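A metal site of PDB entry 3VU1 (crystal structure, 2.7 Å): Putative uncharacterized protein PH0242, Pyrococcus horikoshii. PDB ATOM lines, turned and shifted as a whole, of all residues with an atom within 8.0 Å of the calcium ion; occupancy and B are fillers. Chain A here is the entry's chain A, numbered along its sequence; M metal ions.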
ATOM      1  N   GLY A  72     -22.217  -6.336   2.982  1.00  0.00           N
ATOM      2  CA  GLY A  72     -20.982  -6.284   3.739  1.00  0.00           C
ATOM      3  C   GLY A  72     -20.107  -7.490   3.609  1.00  0.00           C
ATOM      4  O   GLY A  72     -20.079  -8.126   2.566  1.00  0.00           O
ATOM      5  N   ASN A  73     -19.392  -7.823   4.685  1.00  0.00           N
ATOM      6  CA  ASN A  73     -18.332  -8.824   4.619  1.00  0.00           C
ATOM      7  C   ASN A  73     -18.809 -10.187   4.190  1.00  0.00           C
ATOM      8  O   ASN A  73     -18.183 -10.797   3.330  1.00  0.00           O
ATOM      9  CB  ASN A  73     -17.614  -8.952   5.964  1.00  0.00           C
ATOM     10  CG  ASN A  73     -16.569  -7.891   6.166  1.00  0.00           C
ATOM     11  OD1 ASN A  73     -16.038  -7.336   5.201  1.00  0.00           O
ATOM     12  ND2 ASN A  73     -16.257  -7.606   7.409  1.00  0.00           N
ATOM     13  N   GLU A  76     -19.320 -11.277   0.522  1.00  0.00           N
ATOM     14  CA  GLU A  76     -18.151 -11.282  -0.366  1.00  0.00           C
ATOM     15  C   GLU A  76     -17.751 -12.694  -0.769  1.00  0.00           C
ATOM     16  O   GLU A  76     -16.835 -13.307  -0.270  1.00  0.00           O
ATOM     17  CB  GLU A  76     -16.973 -10.507   0.217  1.00  0.00           C
ATOM     18  CG  GLU A  76     -17.114  -8.994   0.063  1.00  0.00           C
ATOM     19  CD  GLU A  76     -15.800  -8.255   0.312  1.00  0.00           C
ATOM     20  OE1 GLU A  76     -14.717  -8.758  -0.093  1.00  0.00           O
ATOM     21  OE2 GLU A  76     -15.856  -7.138   0.911  1.00  0.00           O
ATOM     22  N   PHE A 228     -19.080   0.292   1.850  1.00  0.00           N
ATOM     23  CA  PHE A 228     -19.393  -0.942   1.127  1.00  0.00           C
ATOM     24  C   PHE A 228     -20.133  -0.784  -0.219  1.00  0.00           C
ATOM     25  O   PHE A 228     -19.804  -1.460  -1.208  1.00  0.00           O
ATOM     26  CB  PHE A 228     -20.115  -1.972   2.018  1.00  0.00           C
ATOM     27  CG  PHE A 228     -20.149  -3.341   1.386  1.00  0.00           C
ATOM     28  CD1 PHE A 228     -18.993  -4.141   1.338  1.00  0.00           C
ATOM     29  CD2 PHE A 228     -21.313  -3.807   0.751  1.00  0.00           C
ATOM     30  CE1 PHE A 228     -19.010  -5.375   0.719  1.00  0.00           C
ATOM     31  CE2 PHE A 228     -21.327  -5.048   0.137  1.00  0.00           C
ATOM     32  CZ  PHE A 228     -20.183  -5.832   0.119  1.00  0.00           C
ATOM     33  N   LYS A 231     -17.602   0.530  -2.790  1.00  0.00           N
ATOM     34  CA  LYS A 231     -16.648  -0.498  -3.217  1.00  0.00           C
ATOM     35  C   LYS A 231     -17.320  -1.458  -4.152  1.00  0.00           C
ATOM     36  O   LYS A 231     -16.806  -1.709  -5.256  1.00  0.00           O
ATOM     37  CB  LYS A 231     -16.073  -1.262  -2.048  1.00  0.00           C
ATOM     38  CG  LYS A 231     -15.146  -0.478  -1.138  1.00  0.00           C
ATOM     39  CD  LYS A 231     -15.332  -1.012   0.256  1.00  0.00           C
ATOM     40  CE  LYS A 231     -14.214  -1.952   0.674  1.00  0.00           C
ATOM     41  NZ  LYS A 231     -13.133  -1.197   1.365  1.00  0.00           N
ATOM     42  N   LEU A 232     -18.472  -1.979  -3.722  1.00  0.00           N
ATOM     43  CA  LEU A 232     -19.290  -2.831  -4.583  1.00  0.00           C
ATOM     44  C   LEU A 232     -19.419  -2.305  -6.009  1.00  0.00           C
ATOM     45  O   LEU A 232     -19.230  -3.061  -6.964  1.00  0.00           O
ATOM     46  CB  LEU A 232     -20.672  -3.033  -4.012  1.00  0.00           C
ATOM     47  CG  LEU A 232     -21.501  -4.159  -4.667  1.00  0.00           C
ATOM     48  CD1 LEU A 232     -20.979  -5.541  -4.280  1.00  0.00           C
ATOM     49  CD2 LEU A 232     -22.962  -4.056  -4.273  1.00  0.00           C
ATOM     50  N   ASN A 235     -16.567  -3.115  -8.154  1.00  0.00           N
ATOM     51  CA  ASN A 235     -16.436  -4.545  -8.499  1.00  0.00           C
ATOM     52  C   ASN A 235     -17.426  -5.038  -9.581  1.00  0.00           C
ATOM     53  O   ASN A 235     -17.154  -6.009 -10.289  1.00  0.00           O
ATOM     54  CB  ASN A 235     -16.568  -5.393  -7.255  1.00  0.00           C
ATOM     55  CG  ASN A 235     -15.518  -5.060  -6.248  1.00  0.00           C
ATOM     56  OD1 ASN A 235     -14.328  -5.177  -6.526  1.00  0.00           O
ATOM     57  ND2 ASN A 235     -15.930  -4.600  -5.104  1.00  0.00           N
ATOM     58  N   PRO A 252     -12.839  -8.456  -9.827  1.00  0.00           N
ATOM     59  CA  PRO A 252     -12.546  -8.854  -8.429  1.00  0.00           C
ATOM     60  C   PRO A 252     -11.624  -7.844  -7.720  1.00  0.00           C
ATOM     61  O   PRO A 252     -11.779  -7.612  -6.511  1.00  0.00           O
ATOM     62  CB  PRO A 252     -11.902 -10.235  -8.557  1.00  0.00           C
ATOM     63  CG  PRO A 252     -11.450 -10.336  -9.997  1.00  0.00           C
ATOM     64  CD  PRO A 252     -12.313  -9.418 -10.829  1.00  0.00           C
ATOM     65  N   ILE A 283      -8.643   0.804  -3.054  1.00  0.00           N
ATOM     66  CA  ILE A 283      -8.821  -0.502  -3.650  1.00  0.00           C
ATOM     67  C   ILE A 283      -9.947  -1.284  -2.988  1.00  0.00           C
ATOM     68  O   ILE A 283     -10.062  -1.345  -1.761  1.00  0.00           O
ATOM     69  CB  ILE A 283      -7.502  -1.281  -3.631  1.00  0.00           C
ATOM     70  CG1 ILE A 283      -6.570  -0.640  -4.662  1.00  0.00           C
ATOM     71  CG2 ILE A 283      -7.742  -2.768  -3.878  1.00  0.00           C
ATOM     72  CD1 ILE A 283      -5.179  -1.258  -4.787  1.00  0.00           C
ATOM     73  N   SER A 284     -10.806  -1.860  -3.819  1.00  0.00           N
ATOM     74  CA  SER A 284     -11.796  -2.810  -3.342  1.00  0.00           C
ATOM     75  C   SER A 284     -11.461  -4.211  -3.856  1.00  0.00           C
ATOM     76  O   SER A 284     -11.434  -4.440  -5.062  1.00  0.00           O
ATOM     77  CB  SER A 284     -13.178  -2.378  -3.791  1.00  0.00           C
ATOM     78  OG  SER A 284     -14.100  -3.407  -3.534  1.00  0.00           O
ATOM     79  N   ALA A 285     -11.147  -5.131  -2.945  1.00  0.00           N
ATOM     80  CA  ALA A 285     -10.893  -6.530  -3.320  1.00  0.00           C
ATOM     81  C   ALA A 285     -12.077  -7.399  -2.902  1.00  0.00           C
ATOM     82  O   ALA A 285     -12.430  -7.480  -1.707  1.00  0.00           O
ATOM     83  CB  ALA A 285      -9.596  -7.056  -2.707  1.00  0.00           C
ATOM     84  N   PHE A 286     -12.698  -8.033  -3.894  1.00  0.00           N
ATOM     85  CA  PHE A 286     -13.964  -8.711  -3.669  1.00  0.00           C
ATOM     86  C   PHE A 286     -13.900 -10.258  -3.571  1.00  0.00           C
ATOM     87  O   PHE A 286     -13.823 -10.975  -4.589  1.00  0.00           O
ATOM     88  CB  PHE A 286     -15.011  -8.301  -4.718  1.00  0.00           C
ATOM     89  CG  PHE A 286     -16.404  -8.709  -4.346  1.00  0.00           C
ATOM     90  CD1 PHE A 286     -17.204  -7.872  -3.574  1.00  0.00           C
ATOM     91  CD2 PHE A 286     -16.889  -9.974  -4.705  1.00  0.00           C
ATOM     92  CE1 PHE A 286     -18.473  -8.262  -3.213  1.00  0.00           C
ATOM     93  CE2 PHE A 286     -18.150 -10.377  -4.332  1.00  0.00           C
ATOM     94  CZ  PHE A 286     -18.950  -9.514  -3.580  1.00  0.00           C
ATOM     95  N   GLY A 287     -13.979 -10.779  -2.366  1.00  0.00           N
ATOM     96  CA  GLY A 287     -14.010 -12.229  -2.209  1.00  0.00           C
ATOM     97  C   GLY A 287     -12.681 -12.948  -2.125  1.00  0.00           C
ATOM     98  O   GLY A 287     -12.619 -14.032  -1.554  1.00  0.00           O
ATOM     99  N   ARG A 288     -11.622 -12.403  -2.718  1.00  0.00           N
ATOM    100  CA  ARG A 288     -10.288 -12.980  -2.540  1.00  0.00           C
ATOM    101  C   ARG A 288      -9.191 -11.945  -2.271  1.00  0.00           C
ATOM    102  O   ARG A 288      -9.272 -10.793  -2.718  1.00  0.00           O
ATOM    103  CB  ARG A 288      -9.898 -13.922  -3.695  1.00  0.00           C
ATOM    104  CG  ARG A 288      -9.647 -13.246  -5.017  1.00  0.00           C
ATOM    105  CD  ARG A 288      -8.997 -14.177  -6.048  1.00  0.00           C
ATOM    106  NE  ARG A 288      -9.693 -15.464  -6.076  1.00  0.00           N
ATOM    107  CZ  ARG A 288      -9.186 -16.603  -6.535  1.00  0.00           C
ATOM    108  NH1 ARG A 288      -7.956 -16.650  -7.059  1.00  0.00           N
ATOM    109  NH2 ARG A 288      -9.908 -17.719  -6.480  1.00  0.00           N
ATOM    110  N   ASN A 318      -5.526  -8.011   2.697  1.00  0.00           N
ATOM    111  CA  ASN A 318      -6.753  -8.715   3.083  1.00  0.00           C
ATOM    112  C   ASN A 318      -8.010  -8.130   2.445  1.00  0.00           C
ATOM    113  O   ASN A 318      -8.267  -6.923   2.549  1.00  0.00           O
ATOM    114  CB  ASN A 318      -6.929  -8.678   4.598  1.00  0.00           C
ATOM    115  CG  ASN A 318      -8.020  -9.613   5.077  1.00  0.00           C
ATOM    116  OD1 ASN A 318      -9.207  -9.326   4.983  1.00  0.00           O
ATOM    117  ND2 ASN A 318      -7.616 -10.772   5.568  1.00  0.00           N
ATOM    118  N   HIS A 319      -8.843  -8.990   1.835  1.00  0.00           N
ATOM    119  CA  HIS A 319      -9.982  -8.501   1.073  1.00  0.00           C
ATOM    120  C   HIS A 319     -11.085  -7.998   1.927  1.00  0.00           C
ATOM    121  O   HIS A 319     -12.018  -7.384   1.423  1.00  0.00           O
ATOM    122  CB  HIS A 319     -10.479  -9.529   0.076  1.00  0.00           C
ATOM    123  CG  HIS A 319     -11.212 -10.700   0.694  1.00  0.00           C
ATOM    124  ND1 HIS A 319     -12.543 -10.675   0.943  1.00  0.00           N
ATOM    125  CD2 HIS A 319     -10.767 -11.955   1.078  1.00  0.00           C
ATOM    126  CE1 HIS A 319     -12.925 -11.842   1.480  1.00  0.00           C
ATOM    127  NE2 HIS A 319     -11.832 -12.629   1.559  1.00  0.00           N
ATOM    128  N   LEU A 320     -10.995  -8.225   3.224  1.00  0.00           N
ATOM    129  CA  LEU A 320     -11.954  -7.667   4.196  1.00  0.00           C
ATOM    130  C   LEU A 320     -11.436  -6.420   4.914  1.00  0.00           C
ATOM    131  O   LEU A 320     -12.176  -5.796   5.667  1.00  0.00           O
ATOM    132  CB  LEU A 320     -12.347  -8.710   5.236  1.00  0.00           C
ATOM    133  CG  LEU A 320     -12.964  -9.969   4.637  1.00  0.00           C
ATOM    134  CD1 LEU A 320     -13.018 -11.094   5.673  1.00  0.00           C
ATOM    135  CD2 LEU A 320     -14.340  -9.634   4.055  1.00  0.00           C
ATOM    136  N   GLU A 321     -10.176  -6.063   4.673  1.00  0.00           N
ATOM    137  CA  GLU A 321      -9.531  -4.942   5.360  1.00  0.00           C
ATOM    138  C   GLU A 321      -8.521  -4.255   4.447  1.00  0.00           C
ATOM    139  O   GLU A 321      -7.323  -4.173   4.729  1.00  0.00           O
ATOM    140  CB  GLU A 321      -8.896  -5.402   6.660  1.00  0.00           C
ATOM    141  CG  GLU A 321      -9.885  -5.481   7.813  1.00  0.00           C
ATOM    142  CD  GLU A 321      -9.258  -5.990   9.111  1.00  0.00           C
ATOM    143  OE1 GLU A 321      -9.828  -5.695  10.187  1.00  0.00           O
ATOM    144  OE2 GLU A 321      -8.214  -6.691   9.054  1.00  0.00           O
ATOM    145  N   GLU A 322      -9.031  -3.748   3.337  1.00  0.00           N
ATOM    146  CA  GLU A 322      -8.174  -3.192   2.324  1.00  0.00           C
ATOM    147  C   GLU A 322      -7.794  -1.782   2.722  1.00  0.00           C
ATOM    148  O   GLU A 322      -8.507  -1.131   3.470  1.00  0.00           O
ATOM    149  CB  GLU A 322      -8.855  -3.296   0.951  1.00  0.00           C
ATOM    150  CG  GLU A 322     -10.327  -2.955   1.010  1.00  0.00           C
ATOM    151  CD  GLU A 322     -11.278  -4.133   0.861  1.00  0.00           C
ATOM    152  OE1 GLU A 322     -11.250  -4.806  -0.191  1.00  0.00           O
ATOM    153  OE2 GLU A 322     -12.129  -4.327   1.773  1.00  0.00           O
HETATM  154 CA    CA M   1     -13.648  -6.417  -0.059  1.00  0.00          CA
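OE1 of Glu 76 sits close to N of Gly 287, at 3.1 Å.
OE2 of Glu 322 is in salt-bridge range of NZ of Lys 231.
The calcium ion is bound by the backbone carbonyl oxygen (O) of Ala 285 (2.3 Å), the backbone carbonyl oxygen (O) of His 319 (2.4 Å), the side-chain carboxylate (OE2) of Glu 76 (2.5 Å), the side-chain carboxylate (OE1) of Glu 76 (2.6 Å) and the side-chain carboxylate (OE1) of Glu 322 (2.9 Å).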
